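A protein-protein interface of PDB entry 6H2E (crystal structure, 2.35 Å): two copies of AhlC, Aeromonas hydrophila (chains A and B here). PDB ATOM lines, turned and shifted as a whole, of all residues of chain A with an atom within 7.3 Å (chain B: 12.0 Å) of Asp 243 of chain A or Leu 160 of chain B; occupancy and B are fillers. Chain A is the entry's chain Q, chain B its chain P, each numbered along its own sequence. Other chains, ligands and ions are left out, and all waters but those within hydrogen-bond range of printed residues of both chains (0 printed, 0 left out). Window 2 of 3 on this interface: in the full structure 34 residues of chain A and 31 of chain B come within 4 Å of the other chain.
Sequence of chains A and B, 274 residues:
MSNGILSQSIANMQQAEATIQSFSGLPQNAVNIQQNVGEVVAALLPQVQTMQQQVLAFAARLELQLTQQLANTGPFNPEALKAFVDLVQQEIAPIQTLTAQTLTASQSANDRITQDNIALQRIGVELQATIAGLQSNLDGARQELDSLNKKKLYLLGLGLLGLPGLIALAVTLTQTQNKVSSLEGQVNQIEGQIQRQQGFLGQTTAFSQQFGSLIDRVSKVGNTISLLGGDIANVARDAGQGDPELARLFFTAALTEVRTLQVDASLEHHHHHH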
ATOM      1  N   ASP A 238      26.908  -2.042 -26.081  1.00  0.00           N
ATOM      2  CA  ASP A 238      26.497  -2.572 -27.387  1.00  0.00           C
ATOM      3  C   ASP A 238      25.031  -2.197 -27.658  1.00  0.00           C
ATOM      4  O   ASP A 238      24.747  -1.243 -28.398  1.00  0.00           O
ATOM      5  CB  ASP A 238      26.753  -4.086 -27.453  1.00  0.00           C
ATOM      6  CG  ASP A 238      28.148  -4.526 -27.010  1.00  0.00           C
ATOM      7  OD1 ASP A 238      28.875  -3.703 -26.408  1.00  0.00           O
ATOM      8  OD2 ASP A 238      28.498  -5.699 -27.258  1.00  0.00           O
ATOM      9  N   ASP A 243      25.212  -5.107 -33.336  1.00  0.00           N
ATOM     10  CA  ASP A 243      24.359  -6.294 -33.456  1.00  0.00           C
ATOM     11  C   ASP A 243      23.687  -6.529 -32.109  1.00  0.00           C
ATOM     12  O   ASP A 243      24.232  -7.229 -31.263  1.00  0.00           O
ATOM     13  CB  ASP A 243      25.137  -7.545 -33.891  1.00  0.00           C
ATOM     14  CG  ASP A 243      24.276  -8.778 -34.173  1.00  0.00           C
ATOM     15  OD1 ASP A 243      23.023  -8.641 -34.224  1.00  0.00           O
ATOM     16  OD2 ASP A 243      24.861  -9.884 -34.352  1.00  0.00           O
ATOM     17  N   PRO A 244      22.473  -5.978 -31.880  1.00  0.00           N
ATOM     18  CA  PRO A 244      21.877  -5.976 -30.545  1.00  0.00           C
ATOM     19  C   PRO A 244      21.378  -7.361 -30.090  1.00  0.00           C
ATOM     20  O   PRO A 244      20.886  -7.487 -28.968  1.00  0.00           O
ATOM     21  CB  PRO A 244      20.737  -4.955 -30.681  1.00  0.00           C
ATOM     22  CG  PRO A 244      20.320  -5.061 -32.133  1.00  0.00           C
ATOM     23  CD  PRO A 244      21.593  -5.380 -32.894  1.00  0.00           C
ATOM     24  N   GLU A 245      21.549  -8.393 -30.928  1.00  0.00           N
ATOM     25  CA  GLU A 245      21.340  -9.773 -30.512  1.00  0.00           C
ATOM     26  C   GLU A 245      22.520 -10.293 -29.657  1.00  0.00           C
ATOM     27  O   GLU A 245      22.504 -11.443 -29.198  1.00  0.00           O
ATOM     28  CB  GLU A 245      21.143 -10.664 -31.734  1.00  0.00           C
ATOM     29  CG  GLU A 245      20.621 -12.058 -31.411  1.00  0.00           C
ATOM     30  CD  GLU A 245      19.215 -12.094 -30.827  1.00  0.00           C
ATOM     31  OE1 GLU A 245      18.750 -13.220 -30.473  1.00  0.00           O
ATOM     32  OE2 GLU A 245      18.574 -10.998 -30.751  1.00  0.00           O
ATOM     33  N   LEU A 246      23.551  -9.469 -29.427  1.00  0.00           N
ATOM     34  CA  LEU A 246      24.626  -9.839 -28.486  1.00  0.00           C
ATOM     35  C   LEU A 246      24.075  -9.958 -27.048  1.00  0.00           C
ATOM     36  O   LEU A 246      24.591 -10.731 -26.264  1.00  0.00           O
ATOM     37  CB  LEU A 246      25.746  -8.797 -28.562  1.00  0.00           C
ATOM     38  CG  LEU A 246      26.899  -9.136 -29.507  1.00  0.00           C
ATOM     39  CD1 LEU A 246      28.017  -8.098 -29.382  1.00  0.00           C
ATOM     40  CD2 LEU A 246      27.426 -10.545 -29.244  1.00  0.00           C
ATOM     41  N   ALA A 247      23.069  -9.138 -26.721  1.00  0.00           N
ATOM     42  CA  ALA A 247      22.210  -9.244 -25.531  1.00  0.00           C
ATOM     43  C   ALA A 247      21.917 -10.705 -25.146  1.00  0.00           C
ATOM     44  O   ALA A 247      22.112 -11.073 -24.014  1.00  0.00           O
ATOM     45  CB  ALA A 247      20.944  -8.486 -25.753  1.00  0.00           C
ATOM     46  N   ARG A 248      21.528 -11.563 -26.088  1.00  0.00           N
ATOM     47  CA  ARG A 248      21.215 -12.964 -25.726  1.00  0.00           C
ATOM     48  C   ARG A 248      22.400 -13.601 -24.979  1.00  0.00           C
ATOM     49  O   ARG A 248      22.219 -14.371 -24.002  1.00  0.00           O
ATOM     50  CB  ARG A 248      20.837 -13.746 -26.979  1.00  0.00           C
ATOM     51  CG  ARG A 248      20.511 -15.220 -26.779  1.00  0.00           C
ATOM     52  CD  ARG A 248      19.233 -15.471 -26.031  1.00  0.00           C
ATOM     53  NE  ARG A 248      18.201 -14.584 -26.555  1.00  0.00           N
ATOM     54  CZ  ARG A 248      17.082 -14.977 -27.131  1.00  0.00           C
ATOM     55  NH1 ARG A 248      16.748 -16.254 -27.083  1.00  0.00           N
ATOM     56  NH2 ARG A 248      16.288 -14.085 -27.697  1.00  0.00           N
ATOM     57  N   LEU A 249      23.615 -13.341 -25.465  1.00  0.00           N
ATOM     58  CA  LEU A 249      24.836 -14.031 -24.988  1.00  0.00           C
ATOM     59  C   LEU A 249      25.147 -13.544 -23.570  1.00  0.00           C
ATOM     60  O   LEU A 249      25.375 -14.333 -22.686  1.00  0.00           O
ATOM     61  CB  LEU A 249      25.989 -13.759 -25.964  1.00  0.00           C
ATOM     62  CG  LEU A 249      27.346 -14.424 -25.694  1.00  0.00           C
ATOM     63  CD1 LEU A 249      27.330 -15.904 -26.086  1.00  0.00           C
ATOM     64  CD2 LEU A 249      28.447 -13.700 -26.471  1.00  0.00           C
ATOM     65  N   PHE A 250      25.120 -12.227 -23.374  1.00  0.00           N
ATOM     66  CA  PHE A 250      25.496 -11.627 -22.121  1.00  0.00           C
ATOM     67  C   PHE A 250      24.384 -11.848 -21.086  1.00  0.00           C
ATOM     68  O   PHE A 250      24.669 -11.936 -19.885  1.00  0.00           O
ATOM     69  CB  PHE A 250      25.925 -10.173 -22.345  1.00  0.00           C
ATOM     70  CG  PHE A 250      27.228 -10.093 -23.097  1.00  0.00           C
ATOM     71  CD1 PHE A 250      28.387 -10.640 -22.559  1.00  0.00           C
ATOM     72  CD2 PHE A 250      27.312  -9.495 -24.347  1.00  0.00           C
ATOM     73  CE1 PHE A 250      29.593 -10.596 -23.248  1.00  0.00           C
ATOM     74  CE2 PHE A 250      28.518  -9.457 -25.035  1.00  0.00           C
ATOM     75  CZ  PHE A 250      29.648 -10.022 -24.494  1.00  0.00           C
ATOM     76  N   LYS B 152      33.331 -21.833 -20.159  1.00  0.00           N
ATOM     77  CA  LYS B 152      32.433 -20.671 -20.187  1.00  0.00           C
ATOM     78  C   LYS B 152      33.125 -19.414 -20.729  1.00  0.00           C
ATOM     79  O   LYS B 152      32.528 -18.711 -21.528  1.00  0.00           O
ATOM     80  CB  LYS B 152      31.900 -20.354 -18.791  1.00  0.00           C
ATOM     81  CG  LYS B 152      30.759 -19.347 -18.741  1.00  0.00           C
ATOM     82  CD  LYS B 152      30.851 -18.380 -17.578  1.00  0.00           C
ATOM     83  CE  LYS B 152      30.075 -18.805 -16.355  1.00  0.00           C
ATOM     84  NZ  LYS B 152      30.029 -17.691 -15.381  1.00  0.00           N
ATOM     85  N   LEU B 153      34.338 -19.106 -20.250  1.00  0.00           N
ATOM     86  CA  LEU B 153      35.029 -17.848 -20.630  1.00  0.00           C
ATOM     87  C   LEU B 153      35.467 -17.927 -22.105  1.00  0.00           C
ATOM     88  O   LEU B 153      35.409 -16.928 -22.829  1.00  0.00           O
ATOM     89  CB  LEU B 153      36.216 -17.587 -19.690  1.00  0.00           C
ATOM     90  CG  LEU B 153      35.879 -17.455 -18.203  1.00  0.00           C
ATOM     91  CD1 LEU B 153      37.134 -17.376 -17.348  1.00  0.00           C
ATOM     92  CD2 LEU B 153      34.992 -16.251 -17.912  1.00  0.00           C
ATOM     93  N   TYR B 154      35.866 -19.127 -22.543  1.00  0.00           N
ATOM     94  CA  TYR B 154      36.190 -19.402 -23.943  1.00  0.00           C
ATOM     95  C   TYR B 154      35.012 -18.956 -24.818  1.00  0.00           C
ATOM     96  O   TYR B 154      35.142 -18.019 -25.587  1.00  0.00           O
ATOM     97  CB  TYR B 154      36.516 -20.884 -24.123  1.00  0.00           C
ATOM     98  CG  TYR B 154      37.081 -21.291 -25.464  1.00  0.00           C
ATOM     99  CD1 TYR B 154      36.252 -21.670 -26.514  1.00  0.00           C
ATOM    100  CD2 TYR B 154      38.455 -21.374 -25.667  1.00  0.00           C
ATOM    101  CE1 TYR B 154      36.773 -22.083 -27.734  1.00  0.00           C
ATOM    102  CE2 TYR B 154      38.993 -21.789 -26.879  1.00  0.00           C
ATOM    103  CZ  TYR B 154      38.148 -22.146 -27.918  1.00  0.00           C
ATOM    104  OH  TYR B 154      38.671 -22.545 -29.115  1.00  0.00           O
ATOM    105  N   LEU B 155      33.865 -19.624 -24.629  1.00  0.00           N
ATOM    106  CA  LEU B 155      32.628 -19.443 -25.382  1.00  0.00           C
ATOM    107  C   LEU B 155      32.190 -17.977 -25.374  1.00  0.00           C
ATOM    108  O   LEU B 155      31.858 -17.431 -26.423  1.00  0.00           O
ATOM    109  CB  LEU B 155      31.565 -20.361 -24.774  1.00  0.00           C
ATOM    110  CG  LEU B 155      31.738 -21.845 -25.105  1.00  0.00           C
ATOM    111  CD1 LEU B 155      31.025 -22.757 -24.106  1.00  0.00           C
ATOM    112  CD2 LEU B 155      31.248 -22.130 -26.503  1.00  0.00           C
ATOM    113  N   LEU B 156      32.236 -17.330 -24.204  1.00  0.00           N
ATOM    114  CA  LEU B 156      31.890 -15.892 -24.117  1.00  0.00           C
ATOM    115  C   LEU B 156      32.745 -15.037 -25.070  1.00  0.00           C
ATOM    116  O   LEU B 156      32.281 -14.002 -25.591  1.00  0.00           O
ATOM    117  CB  LEU B 156      32.061 -15.413 -22.670  1.00  0.00           C
ATOM    118  CG  LEU B 156      30.748 -15.056 -21.984  1.00  0.00           C
ATOM    119  CD1 LEU B 156      30.964 -14.646 -20.526  1.00  0.00           C
ATOM    120  CD2 LEU B 156      30.067 -13.936 -22.750  1.00  0.00           C
ATOM    121  N   GLY B 157      34.006 -15.447 -25.259  1.00  0.00           N
ATOM    122  CA  GLY B 157      34.919 -14.816 -26.217  1.00  0.00           C
ATOM    123  C   GLY B 157      34.514 -15.023 -27.674  1.00  0.00           C
ATOM    124  O   GLY B 157      34.851 -14.202 -28.490  1.00  0.00           O
ATOM    125  N   LEU B 158      33.782 -16.102 -27.997  1.00  0.00           N
ATOM    126  CA  LEU B 158      33.426 -16.418 -29.378  1.00  0.00           C
ATOM    127  C   LEU B 158      32.201 -15.648 -29.876  1.00  0.00           C
ATOM    128  O   LEU B 158      31.624 -16.039 -30.911  1.00  0.00           O
ATOM    129  CB  LEU B 158      33.156 -17.916 -29.502  1.00  0.00           C
ATOM    130  CG  LEU B 158      34.340 -18.814 -29.183  1.00  0.00           C
ATOM    131  CD1 LEU B 158      34.134 -20.194 -29.804  1.00  0.00           C
ATOM    132  CD2 LEU B 158      35.641 -18.194 -29.678  1.00  0.00           C
ATOM    133  N   GLY B 159      31.785 -14.578 -29.183  1.00  0.00           N
ATOM    134  CA  GLY B 159      30.500 -13.932 -29.527  1.00  0.00           C
ATOM    135  C   GLY B 159      29.376 -14.958 -29.673  1.00  0.00           C
ATOM    136  O   GLY B 159      29.302 -15.930 -28.894  1.00  0.00           O
ATOM    137  N   LEU B 160      28.504 -14.754 -30.671  1.00  0.00           N
ATOM    138  CA  LEU B 160      27.223 -15.470 -30.822  1.00  0.00           C
ATOM    139  C   LEU B 160      27.458 -16.905 -31.283  1.00  0.00           C
ATOM    140  O   LEU B 160      26.571 -17.764 -31.153  1.00  0.00           O
ATOM    141  CB  LEU B 160      26.346 -14.754 -31.854  1.00  0.00           C
ATOM    142  CG  LEU B 160      25.538 -13.556 -31.349  1.00  0.00           C
ATOM    143  CD1 LEU B 160      24.943 -12.791 -32.508  1.00  0.00           C
ATOM    144  CD2 LEU B 160      24.433 -13.996 -30.401  1.00  0.00           C
ATOM    145  N   LEU B 161      28.641 -17.167 -31.842  1.00  0.00           N
ATOM    146  CA  LEU B 161      29.006 -18.546 -32.230  1.00  0.00           C
ATOM    147  C   LEU B 161      29.088 -19.450 -30.984  1.00  0.00           C
ATOM    148  O   LEU B 161      28.888 -20.678 -31.056  1.00  0.00           O
ATOM    149  CB  LEU B 161      30.321 -18.493 -33.012  1.00  0.00           C
ATOM    150  CG  LEU B 161      30.277 -17.563 -34.226  1.00  0.00           C
ATOM    151  CD1 LEU B 161      31.600 -17.577 -34.973  1.00  0.00           C
ATOM    152  CD2 LEU B 161      29.124 -17.922 -35.163  1.00  0.00           C
ATOM    153  N   GLY B 162      29.313 -18.830 -29.823  1.00  0.00           N
ATOM    154  CA  GLY B 162      29.446 -19.563 -28.569  1.00  0.00           C
ATOM    155  C   GLY B 162      28.168 -19.590 -27.761  1.00  0.00           C
ATOM    156  O   GLY B 162      28.147 -20.160 -26.699  1.00  0.00           O
ATOM    157  N   LEU B 163      27.080 -19.028 -28.296  1.00  0.00           N
ATOM    158  CA  LEU B 163      25.843 -19.034 -27.595  1.00  0.00           C
ATOM    159  C   LEU B 163      25.294 -20.457 -27.483  1.00  0.00           C
ATOM    160  O   LEU B 163      24.882 -20.868 -26.412  1.00  0.00           O
ATOM    161  CB  LEU B 163      24.845 -18.098 -28.274  1.00  0.00           C
ATOM    162  CG  LEU B 163      23.465 -18.110 -27.625  1.00  0.00           C
ATOM    163  CD1 LEU B 163      23.576 -17.775 -26.139  1.00  0.00           C
ATOM    164  CD2 LEU B 163      22.531 -17.146 -28.337  1.00  0.00           C
ATOM    165  N   PRO B 164      25.202 -21.257 -28.565  1.00  0.00           N
ATOM    166  CA  PRO B 164      24.735 -22.630 -28.427  1.00  0.00           C
ATOM    167  C   PRO B 164      25.537 -23.399 -27.365  1.00  0.00           C
ATOM    168  O   PRO B 164      24.965 -24.088 -26.544  1.00  0.00           O
ATOM    169  CB  PRO B 164      24.952 -23.186 -29.847  1.00  0.00           C
ATOM    170  CG  PRO B 164      24.785 -21.980 -30.748  1.00  0.00           C
ATOM    171  CD  PRO B 164      25.449 -20.870 -29.967  1.00  0.00           C
ATOM    172  N   GLY B 165      26.868 -23.262 -27.380  1.00  0.00           N
ATOM    173  CA  GLY B 165      27.751 -23.941 -26.397  1.00  0.00           C
ATOM    174  C   GLY B 165      27.428 -23.496 -24.980  1.00  0.00           C
ATOM    175  O   GLY B 165      27.357 -24.287 -24.069  1.00  0.00           O
ATOM    176  N   LEU B 166      27.158 -22.202 -24.828  1.00  0.00           N
ATOM    177  CA  LEU B 166      27.048 -21.574 -23.542  1.00  0.00           C
ATOM    178  C   LEU B 166      25.758 -22.061 -22.864  1.00  0.00           C
ATOM    179  O   LEU B 166      25.734 -22.303 -21.674  1.00  0.00           O
ATOM    180  CB  LEU B 166      27.102 -20.050 -23.740  1.00  0.00           C
ATOM    181  CG  LEU B 166      26.967 -19.207 -22.472  1.00  0.00           C
ATOM    182  CD1 LEU B 166      28.045 -19.573 -21.481  1.00  0.00           C
ATOM    183  CD2 LEU B 166      27.024 -17.720 -22.758  1.00  0.00           C
ATOM    184  N   ILE B 167      24.702 -22.272 -23.645  1.00  0.00           N
ATOM    185  CA  ILE B 167      23.378 -22.689 -23.103  1.00  0.00           C
ATOM    186  C   ILE B 167      23.449 -24.123 -22.558  1.00  0.00           C
ATOM    187  O   ILE B 167      23.022 -24.364 -21.435  1.00  0.00           O
ATOM    188  CB  ILE B 167      22.288 -22.510 -24.175  1.00  0.00           C
ATOM    189  CG1 ILE B 167      22.047 -21.019 -24.445  1.00  0.00           C
ATOM    190  CG2 ILE B 167      21.006 -23.243 -23.780  1.00  0.00           C
ATOM    191  CD1 ILE B 167      21.202 -20.731 -25.700  1.00  0.00           C
ATOM    192  N   ALA B 168      23.985 -25.042 -23.365  1.00  0.00           N
ATOM    193  CA  ALA B 168      24.245 -26.432 -23.030  1.00  0.00           C
ATOM    194  C   ALA B 168      25.162 -26.562 -21.799  1.00  0.00           C
ATOM    195  O   ALA B 168      24.937 -27.383 -20.910  1.00  0.00           O
ATOM    196  CB  ALA B 168      24.853 -27.068 -24.249  1.00  0.00           C
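No position is printed for both chains.
Of the 8 pairs that touch across the chains among the printed residues, none has its exchanged pair printed and touching as well.
Asp 243 of chain A touches Leu 160 of chain B (OD2 to CD1, 3.4 Å).
Leu 160 of chain B touches Glu 245 of chain A (CD2 to O, 3.4 Å).
Leu 163 of chain B touches Arg 248 of chain A (CD2 to CG, 3.2 Å).
Leu 249 of chain A touches Leu 156 of chain B (CD2 to O, 3.9 Å).
Gly 159 of chain B touches Leu 249 of chain A (O to CD2, 3.4 Å).
Leu 249 of chain A touches Leu 163 of chain B (CD1 to CA, 3.8 Å).
Leu 166 of chain B touches Leu 249 of chain A (CD2 to O, 3.8 Å).
Leu 156 of chain B touches Phe 250 of chain A.
The guanidinium group (NH2) of Arg 248 of chain A is in salt-bridge range of the side-chain carboxylate (OE1) of Glu 245 of chain A (3.8 Å).
Of chain B, only Leu 160 (3.4 Å) comes within 4 Å of Asp 243 of chain A.
Leu 160 of chain B touches just these residues of chain A: Asp 243 and Glu 245.
No residue of chain B comes within 4 Å of Asp 238 of chain A.
No residue of chain B comes within 4 Å of Leu 246 of chain A.
Ala 247 of chain A touches none of the printed residues of chain B.
Leu 249 of chain A touches just these residues of chain B: Leu 156 (3.9 Å), Gly 159 (3.4 Å), Leu 163 (3.8 Å) and Leu 166 (3.8 Å).
Of the printed residues of chain B, Arg 248 of chain A touches Leu 163 (3.2 Å).
Printed residues of chain A within 4 Å of Leu 156 of chain B: Leu 249 and Phe 250.
Of the printed residues of chain A, Leu 163 of chain B touches Arg 248 (3.2 Å) and Leu 249 (3.8 Å).
Of the printed residues of chain A, Gly 159 of chain B touches Leu 249 (3.4 Å).
Printed residues of chain B within 4 Å of Phe 250 of chain A: Leu 156.
Leu 158 of chain B touches none of the printed residues of chain A.
Leu 153 of chain B touches none of the printed residues of chain A.
The nearest residue of chain B that does not touch Asp 243 of chain A is Gly 159 of chain B (8.2 Å).
The nearest printed residue of chain B that does not touch Arg 248 of chain A is Leu 160 of chain B (5.0 Å).
Printed residues of chain B that touch a printed residue of chain A: Leu 156, Gly 159, Leu 160, Leu 163 and Leu 166.
Of the 9 printed residues of chain A, 5 touch a printed residue of chain B.
Among the printed residues, no Asp or Glu carboxylate lies within 4 Å of a Lys or Arg side-chain nitrogen of the other chain.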
